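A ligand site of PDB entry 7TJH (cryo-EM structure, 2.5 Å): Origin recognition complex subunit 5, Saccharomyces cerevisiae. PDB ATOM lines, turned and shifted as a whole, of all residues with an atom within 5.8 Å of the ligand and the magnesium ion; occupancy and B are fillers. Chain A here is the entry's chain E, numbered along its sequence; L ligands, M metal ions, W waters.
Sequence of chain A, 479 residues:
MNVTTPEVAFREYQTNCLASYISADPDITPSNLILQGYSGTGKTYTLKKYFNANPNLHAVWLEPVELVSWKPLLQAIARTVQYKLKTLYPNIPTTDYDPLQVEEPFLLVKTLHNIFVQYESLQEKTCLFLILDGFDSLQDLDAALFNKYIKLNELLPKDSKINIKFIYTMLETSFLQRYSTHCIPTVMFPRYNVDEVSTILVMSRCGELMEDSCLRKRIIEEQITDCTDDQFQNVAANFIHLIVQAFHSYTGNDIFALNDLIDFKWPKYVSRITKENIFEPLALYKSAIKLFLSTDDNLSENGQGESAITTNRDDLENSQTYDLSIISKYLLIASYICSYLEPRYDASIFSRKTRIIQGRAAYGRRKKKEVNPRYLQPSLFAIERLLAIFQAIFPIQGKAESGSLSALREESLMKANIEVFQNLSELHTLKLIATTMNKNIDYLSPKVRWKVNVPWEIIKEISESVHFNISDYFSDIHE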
ATOM      1  N   VAL A   8       3.695  -4.441  38.869  1.00  0.00           N
ATOM      2  CA  VAL A   8       3.803  -3.979  37.494  1.00  0.00           C
ATOM      3  C   VAL A   8       3.737  -2.457  37.526  1.00  0.00           C
ATOM      4  O   VAL A   8       2.754  -1.899  38.032  1.00  0.00           O
ATOM      5  CB  VAL A   8       2.704  -4.570  36.600  1.00  0.00           C
ATOM      6  CG1 VAL A   8       2.866  -4.078  35.173  1.00  0.00           C
ATOM      7  CG2 VAL A   8       2.740  -6.082  36.658  1.00  0.00           C
ATOM      8  N   ALA A   9       4.771  -1.817  36.995  1.00  0.00           N
ATOM      9  CA  ALA A   9       4.874  -0.359  37.059  1.00  0.00           C
ATOM     10  C   ALA A   9       3.789   0.301  36.214  1.00  0.00           C
ATOM     11  O   ALA A   9       3.520  -0.123  35.085  1.00  0.00           O
ATOM     12  CB  ALA A   9       6.260   0.081  36.585  1.00  0.00           C
ATOM     13  N   PHE A  10       3.154   1.315  36.799  1.00  0.00           N
ATOM     14  CA  PHE A  10       2.073   2.127  36.245  1.00  0.00           C
ATOM     15  C   PHE A  10       0.808   1.330  35.920  1.00  0.00           C
ATOM     16  O   PHE A  10      -0.083   1.848  35.245  1.00  0.00           O
ATOM     17  CB  PHE A  10       2.520   2.922  35.012  1.00  0.00           C
ATOM     18  CG  PHE A  10       3.910   3.468  35.125  1.00  0.00           C
ATOM     19  CD1 PHE A  10       4.204   4.439  36.060  1.00  0.00           C
ATOM     20  CD2 PHE A  10       4.921   2.999  34.296  1.00  0.00           C
ATOM     21  CE1 PHE A  10       5.486   4.938  36.171  1.00  0.00           C
ATOM     22  CE2 PHE A  10       6.203   3.497  34.407  1.00  0.00           C
ATOM     23  CZ  PHE A  10       6.486   4.460  35.343  1.00  0.00           C
ATOM     24  N   ARG A  11       0.699   0.087  36.387  1.00  0.00           N
ATOM     25  CA  ARG A  11      -0.480  -0.741  36.190  1.00  0.00           C
ATOM     26  C   ARG A  11      -0.930  -1.391  37.497  1.00  0.00           C
ATOM     27  O   ARG A  11      -1.397  -2.522  37.505  1.00  0.00           O
ATOM     28  CB  ARG A  11      -0.231  -1.825  35.139  1.00  0.00           C
ATOM     29  CG  ARG A  11       0.200  -1.326  33.762  1.00  0.00           C
ATOM     30  CD  ARG A  11      -0.971  -0.867  32.909  1.00  0.00           C
ATOM     31  NE  ARG A  11      -1.286   0.537  33.121  1.00  0.00           N
ATOM     32  CZ  ARG A  11      -1.976   1.291  32.264  1.00  0.00           C
ATOM     33  NH1 ARG A  11      -2.385   0.813  31.104  1.00  0.00           N
ATOM     34  NH2 ARG A  11      -2.243   2.552  32.591  1.00  0.00           N
ATOM     35  N   GLY A  37      -8.200  -2.067  26.174  1.00  0.00           N
ATOM     36  CA  GLY A  37      -7.233  -0.996  26.024  1.00  0.00           C
ATOM     37  C   GLY A  37      -6.735  -0.950  24.602  1.00  0.00           C
ATOM     38  O   GLY A  37      -6.822  -1.940  23.875  1.00  0.00           O
ATOM     39  N   TYR A  38      -6.208   0.193  24.223  1.00  0.00           N
ATOM     40  CA  TYR A  38      -5.699   0.344  22.870  1.00  0.00           C
ATOM     41  C   TYR A  38      -4.303  -0.252  22.779  1.00  0.00           C
ATOM     42  O   TYR A  38      -3.800  -0.876  23.714  1.00  0.00           O
ATOM     43  CB  TYR A  38      -5.775   1.799  22.437  1.00  0.00           C
ATOM     44  CG  TYR A  38      -7.208   2.235  22.208  1.00  0.00           C
ATOM     45  CD1 TYR A  38      -7.795   2.089  20.961  1.00  0.00           C
ATOM     46  CD2 TYR A  38      -7.975   2.730  23.254  1.00  0.00           C
ATOM     47  CE1 TYR A  38      -9.116   2.466  20.758  1.00  0.00           C
ATOM     48  CE2 TYR A  38      -9.290   3.099  23.053  1.00  0.00           C
ATOM     49  CZ  TYR A  38      -9.849   2.963  21.807  1.00  0.00           C
ATOM     50  OH  TYR A  38     -11.158   3.338  21.612  1.00  0.00           O
ATOM     51  N   SER A  39      -3.674  -0.090  21.614  1.00  0.00           N
ATOM     52  CA  SER A  39      -2.445  -0.820  21.309  1.00  0.00           C
ATOM     53  C   SER A  39      -1.279  -0.317  22.152  1.00  0.00           C
ATOM     54  O   SER A  39      -1.071   0.889  22.290  1.00  0.00           O
ATOM     55  CB  SER A  39      -2.116  -0.690  19.823  1.00  0.00           C
ATOM     56  OG  SER A  39      -0.976  -1.446  19.486  1.00  0.00           O
ATOM     57  N   GLY A  40      -0.551  -1.263  22.737  1.00  0.00           N
ATOM     58  CA  GLY A  40       0.612  -0.918  23.535  1.00  0.00           C
ATOM     59  C   GLY A  40       0.312  -0.385  24.908  1.00  0.00           C
ATOM     60  O   GLY A  40       1.123   0.352  25.473  1.00  0.00           O
ATOM     61  N   THR A  41      -0.849  -0.726  25.478  1.00  0.00           N
ATOM     62  CA  THR A  41      -1.211  -0.267  26.808  1.00  0.00           C
ATOM     63  C   THR A  41      -0.857  -1.262  27.896  1.00  0.00           C
ATOM     64  O   THR A  41      -1.258  -1.073  29.048  1.00  0.00           O
ATOM     65  CB  THR A  41      -2.709   0.065  26.851  1.00  0.00           C
ATOM     66  OG1 THR A  41      -3.462  -1.008  26.270  1.00  0.00           O
ATOM     67  CG2 THR A  41      -2.969   1.341  26.074  1.00  0.00           C
ATOM     68  N   GLY A  42      -0.126  -2.324  27.551  1.00  0.00           N
ATOM     69  CA  GLY A  42       0.406  -3.221  28.557  1.00  0.00           C
ATOM     70  C   GLY A  42      -0.564  -4.209  29.169  1.00  0.00           C
ATOM     71  O   GLY A  42      -0.402  -4.583  30.327  1.00  0.00           O
ATOM     72  N   LYS A  43      -1.511  -4.644  28.360  1.00  0.00           N
ATOM     73  CA  LYS A  43      -2.583  -5.590  28.725  1.00  0.00           C
ATOM     74  C   LYS A  43      -2.029  -6.995  28.742  1.00  0.00           C
ATOM     75  O   LYS A  43      -2.197  -7.635  29.740  1.00  0.00           O
ATOM     76  CB  LYS A  43      -3.679  -5.503  27.648  1.00  0.00           C
ATOM     77  CG  LYS A  43      -4.377  -4.181  27.447  1.00  0.00           C
ATOM     78  CD  LYS A  43      -5.643  -4.317  26.611  1.00  0.00           C
ATOM     79  CE  LYS A  43      -5.421  -4.901  25.233  1.00  0.00           C
ATOM     80  NZ  LYS A  43      -4.644  -4.018  24.343  1.00  0.00           N
ATOM     81  N   THR A  44      -1.384  -7.394  27.691  1.00  0.00           N
ATOM     82  CA  THR A  44      -0.703  -8.686  27.533  1.00  0.00           C
ATOM     83  C   THR A  44       0.453  -8.810  28.520  1.00  0.00           C
ATOM     84  O   THR A  44       0.635  -9.862  29.136  1.00  0.00           O
ATOM     85  CB  THR A  44      -0.197  -8.845  26.097  1.00  0.00           C
ATOM     86  OG1 THR A  44      -1.297  -8.775  25.188  1.00  0.00           O
ATOM     87  CG2 THR A  44       0.519 -10.172  25.897  1.00  0.00           C
ATOM     88  N   TYR A  45       1.198  -7.719  28.715  1.00  0.00           N
ATOM     89  CA  TYR A  45       2.339  -7.715  29.636  1.00  0.00           C
ATOM     90  C   TYR A  45       1.900  -7.958  31.076  1.00  0.00           C
ATOM     91  O   TYR A  45       2.500  -8.780  31.787  1.00  0.00           O
ATOM     92  CB  TYR A  45       3.084  -6.384  29.523  1.00  0.00           C
ATOM     93  CG  TYR A  45       4.253  -6.207  30.474  1.00  0.00           C
ATOM     94  CD1 TYR A  45       5.487  -6.781  30.200  1.00  0.00           C
ATOM     95  CD2 TYR A  45       4.110  -5.465  31.643  1.00  0.00           C
ATOM     96  CE1 TYR A  45       6.552  -6.628  31.067  1.00  0.00           C
ATOM     97  CE2 TYR A  45       5.170  -5.316  32.518  1.00  0.00           C
ATOM     98  CZ  TYR A  45       6.383  -5.899  32.222  1.00  0.00           C
ATOM     99  OH  TYR A  45       7.442  -5.739  33.087  1.00  0.00           O
ATOM    100  N   THR A  46       0.838  -7.281  31.526  1.00  0.00           N
ATOM    101  CA  THR A  46       0.449  -7.467  32.923  1.00  0.00           C
ATOM    102  C   THR A  46      -0.339  -8.760  33.127  1.00  0.00           C
ATOM    103  O   THR A  46      -0.294  -9.320  34.230  1.00  0.00           O
ATOM    104  CB  THR A  46      -0.317  -6.247  33.447  1.00  0.00           C
ATOM    105  OG1 THR A  46      -0.318  -6.258  34.875  1.00  0.00           O
ATOM    106  CG2 THR A  46      -1.735  -6.233  32.990  1.00  0.00           C
ATOM    107  N   ASP A 133      -6.699 -13.422  23.582  1.00  0.00           N
ATOM    108  CA  ASP A 133      -5.924 -12.192  23.546  1.00  0.00           C
ATOM    109  C   ASP A 133      -6.058 -11.561  22.165  1.00  0.00           C
ATOM    110  O   ASP A 133      -5.364 -11.935  21.221  1.00  0.00           O
ATOM    111  CB  ASP A 133      -4.463 -12.473  23.895  1.00  0.00           C
ATOM    112  CG  ASP A 133      -3.692 -11.206  24.299  1.00  0.00           C
ATOM    113  OD1 ASP A 133      -4.238 -10.091  24.190  1.00  0.00           O
ATOM    114  OD2 ASP A 133      -2.529 -11.354  24.730  1.00  0.00           O
ATOM    115  N   LEU A 171      -9.605  -4.224  21.855  1.00  0.00           N
ATOM    116  CA  LEU A 171      -8.878  -3.001  21.515  1.00  0.00           C
ATOM    117  C   LEU A 171      -9.779  -1.778  21.580  1.00  0.00           C
ATOM    118  O   LEU A 171      -9.450  -0.801  22.258  1.00  0.00           O
ATOM    119  CB  LEU A 171      -8.248  -3.142  20.122  1.00  0.00           C
ATOM    120  CG  LEU A 171      -6.835  -3.729  20.117  1.00  0.00           C
ATOM    121  CD1 LEU A 171      -6.450  -4.200  18.718  1.00  0.00           C
ATOM    122  CD2 LEU A 171      -5.829  -2.727  20.644  1.00  0.00           C
ATOM    123  N   TYR A 192      -0.656   5.245  28.255  1.00  0.00           N
ATOM    124  CA  TYR A 192       0.372   5.808  29.105  1.00  0.00           C
ATOM    125  C   TYR A 192       0.616   7.275  28.740  1.00  0.00           C
ATOM    126  O   TYR A 192       0.401   7.694  27.612  1.00  0.00           O
ATOM    127  CB  TYR A 192       1.674   5.022  28.974  1.00  0.00           C
ATOM    128  CG  TYR A 192       1.608   3.576  29.430  1.00  0.00           C
ATOM    129  CD1 TYR A 192       1.395   3.255  30.765  1.00  0.00           C
ATOM    130  CD2 TYR A 192       1.787   2.534  28.517  1.00  0.00           C
ATOM    131  CE1 TYR A 192       1.353   1.937  31.185  1.00  0.00           C
ATOM    132  CE2 TYR A 192       1.739   1.210  28.931  1.00  0.00           C
ATOM    133  CZ  TYR A 192       1.530   0.919  30.268  1.00  0.00           C
ATOM    134  OH  TYR A 192       1.475  -0.384  30.685  1.00  0.00           O
ATOM    135  N   ILE A 200       9.144   3.200  30.812  1.00  0.00           N
ATOM    136  CA  ILE A 200       9.016   1.863  30.242  1.00  0.00           C
ATOM    137  C   ILE A 200      10.082   1.617  29.184  1.00  0.00           C
ATOM    138  O   ILE A 200      10.715   0.553  29.155  1.00  0.00           O
ATOM    139  CB  ILE A 200       7.584   1.649  29.701  1.00  0.00           C
ATOM    140  CG1 ILE A 200       6.601   1.422  30.856  1.00  0.00           C
ATOM    141  CG2 ILE A 200       7.508   0.479  28.725  1.00  0.00           C
ATOM    142  CD1 ILE A 200       5.149   1.677  30.476  1.00  0.00           C
ATOM    143  N   MET A 203      13.547   1.160  31.046  1.00  0.00           N
ATOM    144  CA  MET A 203      13.671  -0.098  31.758  1.00  0.00           C
ATOM    145  C   MET A 203      13.553  -1.312  30.851  1.00  0.00           C
ATOM    146  O   MET A 203      13.956  -2.408  31.248  1.00  0.00           O
ATOM    147  CB  MET A 203      12.624  -0.189  32.876  1.00  0.00           C
ATOM    148  CG  MET A 203      11.209  -0.477  32.400  1.00  0.00           C
ATOM    149  SD  MET A 203       9.942   0.053  33.579  1.00  0.00           S
ATOM    150  CE  MET A 203       9.971  -1.302  34.747  1.00  0.00           C
ATOM    151  N   SER A 204      13.037  -1.146  29.635  1.00  0.00           N
ATOM    152  CA  SER A 204      12.960  -2.255  28.698  1.00  0.00           C
ATOM    153  C   SER A 204      14.088  -2.258  27.675  1.00  0.00           C
ATOM    154  O   SER A 204      14.394  -3.321  27.122  1.00  0.00           O
ATOM    155  CB  SER A 204      11.620  -2.224  27.942  1.00  0.00           C
ATOM    156  OG  SER A 204      11.467  -1.035  27.204  1.00  0.00           O
ATOM    157  N   ILE A 255       4.589   2.916  22.235  1.00  0.00           N
ATOM    158  CA  ILE A 255       5.802   2.212  22.630  1.00  0.00           C
ATOM    159  C   ILE A 255       6.475   1.573  21.414  1.00  0.00           C
ATOM    160  O   ILE A 255       7.706   1.605  21.279  1.00  0.00           O
ATOM    161  CB  ILE A 255       5.478   1.182  23.727  1.00  0.00           C
ATOM    162  CG1 ILE A 255       4.911   1.884  24.962  1.00  0.00           C
ATOM    163  CG2 ILE A 255       6.711   0.361  24.115  1.00  0.00           C
ATOM    164  CD1 ILE A 255       4.676   0.977  26.160  1.00  0.00           C
ATOM    165  N   PHE A 256       5.684   1.002  20.498  1.00  0.00           N
ATOM    166  CA  PHE A 256       6.235   0.271  19.360  1.00  0.00           C
ATOM    167  C   PHE A 256       6.951   1.202  18.386  1.00  0.00           C
ATOM    168  O   PHE A 256       8.049   0.876  17.913  1.00  0.00           O
ATOM    169  CB  PHE A 256       5.130  -0.483  18.624  1.00  0.00           C
ATOM    170  CG  PHE A 256       4.289  -1.364  19.515  1.00  0.00           C
ATOM    171  CD1 PHE A 256       4.863  -2.365  20.276  1.00  0.00           C
ATOM    172  CD2 PHE A 256       2.912  -1.196  19.560  1.00  0.00           C
ATOM    173  CE1 PHE A 256       4.086  -3.174  21.088  1.00  0.00           C
ATOM    174  CE2 PHE A 256       2.123  -2.001  20.377  1.00  0.00           C
ATOM    175  CZ  PHE A 256       2.714  -2.990  21.131  1.00  0.00           C
ATOM    176  N   ASN A 259      10.164   2.385  19.926  1.00  0.00           N
ATOM    177  CA  ASN A 259      11.114   1.285  19.886  1.00  0.00           C
ATOM    178  C   ASN A 259      11.742   1.147  18.507  1.00  0.00           C
ATOM    179  O   ASN A 259      12.955   0.918  18.380  1.00  0.00           O
ATOM    180  CB  ASN A 259      10.416  -0.017  20.286  1.00  0.00           C
ATOM    181  CG  ASN A 259      10.462  -0.277  21.769  1.00  0.00           C
ATOM    182  OD1 ASN A 259      11.430   0.065  22.444  1.00  0.00           O
ATOM    183  ND2 ASN A 259       9.408  -0.881  22.299  1.00  0.00           N
HETATM  184  P1  LIG L   1      -1.529  -4.915  21.637  1.00  0.00           P
HETATM  185  O1  LIG L   1      -2.976  -4.610  21.725  1.00  0.00           O
HETATM  186  O2  LIG L   1      -0.839  -4.252  20.455  1.00  0.00           O
HETATM  187  O3  LIG L   1      -1.211  -6.400  21.627  1.00  0.00           O
HETATM  188  P2  LIG L   1      -0.791  -4.470  24.493  1.00  0.00           P
HETATM  189  O4  LIG L   1      -1.688  -3.477  25.111  1.00  0.00           O
HETATM  190  O5  LIG L   1      -1.098  -5.917  24.828  1.00  0.00           O
HETATM  191  O6  LIG L   1      -0.762  -4.357  22.913  1.00  0.00           O
HETATM  192  P3  LIG L   1       1.962  -5.056  25.383  1.00  0.00           P
HETATM  193  O7  LIG L   1       2.389  -6.043  24.358  1.00  0.00           O
HETATM  194  O8  LIG L   1       1.545  -5.690  26.698  1.00  0.00           O
HETATM  195  O9  LIG L   1       0.736  -4.206  24.875  1.00  0.00           O
HETATM  196  O10 LIG L   1       3.084  -3.978  25.669  1.00  0.00           O
HETATM  197  C1  LIG L   1       4.155  -3.732  24.734  1.00  0.00           C
HETATM  198  C2  LIG L   1       5.483  -3.865  25.435  1.00  0.00           C
HETATM  199  O11 LIG L   1       5.721  -2.695  26.244  1.00  0.00           O
HETATM  200  C3  LIG L   1       5.619  -5.040  26.400  1.00  0.00           C
HETATM  201  O12 LIG L   1       6.028  -6.209  25.708  1.00  0.00           O
HETATM  202  C4  LIG L   1       6.702  -4.550  27.361  1.00  0.00           C
HETATM  203  O13 LIG L   1       8.010  -4.754  26.856  1.00  0.00           O
HETATM  204  C5  LIG L   1       6.402  -3.049  27.435  1.00  0.00           C
HETATM  205  N1  LIG L   1       5.565  -2.653  28.572  1.00  0.00           N
HETATM  206  C6  LIG L   1       4.236  -2.333  28.544  1.00  0.00           C
HETATM  207  N2  LIG L   1       3.744  -2.006  29.707  1.00  0.00           N
HETATM  208  C7  LIG L   1       4.826  -2.115  30.571  1.00  0.00           C
HETATM  209  C8  LIG L   1       4.965  -1.907  31.950  1.00  0.00           C
HETATM  210  N3  LIG L   1       3.967  -1.525  32.752  1.00  0.00           N
HETATM  211  N4  LIG L   1       6.192  -2.106  32.496  1.00  0.00           N
HETATM  212  C9  LIG L   1       7.190  -2.499  31.703  1.00  0.00           C
HETATM  213  N5  LIG L   1       7.176  -2.734  30.389  1.00  0.00           N
HETATM  214  C10 LIG L   1       5.957  -2.518  29.884  1.00  0.00           C
HETATM  215 MG    MG M   1      -1.272  -7.667  23.405  1.00  0.00          MG
HETATM  216  O   HOH W   1      -3.411  -7.477  23.701  1.00  0.00           O
HETATM  217  O   HOH W   2      -4.461  -6.642  21.294  1.00  0.00           O
HETATM  218  O   HOH W   3      -1.577  -9.812  21.810  1.00  0.00           O
HETATM  219  O   HOH W   4       0.981  -7.542  23.165  1.00  0.00           O
HETATM  220  O   HOH W   5      -0.344  -7.997  19.355  1.00  0.00           O
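O5 of the ligand sits close to N of Thr 44.
A nitrogen (N3) of the ligand lies within hydrogen-bond range of the backbone carbonyl oxygen (O) of Ala 9, at 2.8 Å.
An oxygen (O8) of the ligand sits at hydrogen-bond distance from the backbone NH of Tyr 45.
O4 of the ligand sits at hydrogen-bond distance from N of Thr 41.
The side-chain hydroxyl (OG1) of Thr 41 is in hydrogen-bond range of an oxygen (O4) of the ligand, at 3.3 Å.
OH of Tyr 192 lies within hydrogen-bond range of N2 of the ligand (3.0 Å).
The side-chain hydroxyl of Ser 39 sits at hydrogen-bond distance from an oxygen (O2) of the ligand, 3.0 Å away.
The backbone NH (N) of Lys 43 sits at hydrogen-bond distance from an oxygen (O4) of the ligand.
NZ of Lys 43 lies within salt-bridge range of O4 of the ligand (3.1 Å).
The backbone NH (N) of Gly 40 sits at hydrogen-bond distance from an oxygen (O6) of the ligand (3.1 Å).
An oxygen (O4) of the ligand is in hydrogen-bond range of the backbone NH (N) of Gly 42 (3.1 Å).
The side-chain hydroxyl (OG1) of Thr 44 sits close to the side-chain carboxylate (OD2) of Asp 133 (2.9 Å).
OH of Tyr 192 lies within hydrogen-bond range of O of Thr 41 (3.3 Å).
OG1 of Thr 41 sits at hydrogen-bond distance from O of Tyr 38, 2.6 Å away.
NH1 of Arg 11 is in hydrogen-bond range of O of Thr 41 (3.0 Å).
NZ of Lys 43 is in hydrogen-bond range of O of Tyr 38, at 3.3 Å.
The side-chain amino group (NZ) of Lys 43 is in hydrogen-bond range of the backbone carbonyl oxygen (O) of Gly 37, at 3.0 Å.
O of Ile 200 lies within hydrogen-bond range of OG of Ser 204, 2.6 Å away.
ND2 of Asn 259 sits at hydrogen-bond distance from O of Ile 255, at 3.2 Å.
Val 8 touches the ligand (CG1 to N3, 3.7 Å).
CG of Arg 11 touches N3 of the ligand, at 3.9 Å.
Tyr 38 touches the ligand (O to O4, 3.6 Å).
Leu 171 touches the ligand.
CG2 of Ile 200 touches C10 of the ligand, 3.6 Å away.
Ile 255 touches the ligand (CD1 to O11, 3.8 Å).
Phe 256 touches the ligand.
Hydrophobic or aromatic side chains within 4 Å of the ligand: Val 8, Tyr 45, Leu 171, Tyr 192, Ile 200, Ile 255 and Phe 256.
Of the 23 residues printed, 16 come within 4 Å of the ligand.
Along chain A the residues within 4 Å of the ligand span positions 8 to 256.
The nearest printed residue that does not touch the ligand is Met 203 (4.2 Å).
Merely in contact with the magnesium ion: Asp 133.
The nearest printed residue that does not touch the magnesium ion is Lys 43 (5.1 Å).
The magnesium ion is bound by OG1 of Thr 44 (2.1 Å), water W1 (2.2 Å), O3 of the ligand (2.2 Å), O5 of the ligand (2.3 Å) and water W4 (2.3 Å).
The magnesium ion has five donor atoms within binding distance.
Slightly farther from the magnesium ion lies water W3 (2.7 Å).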
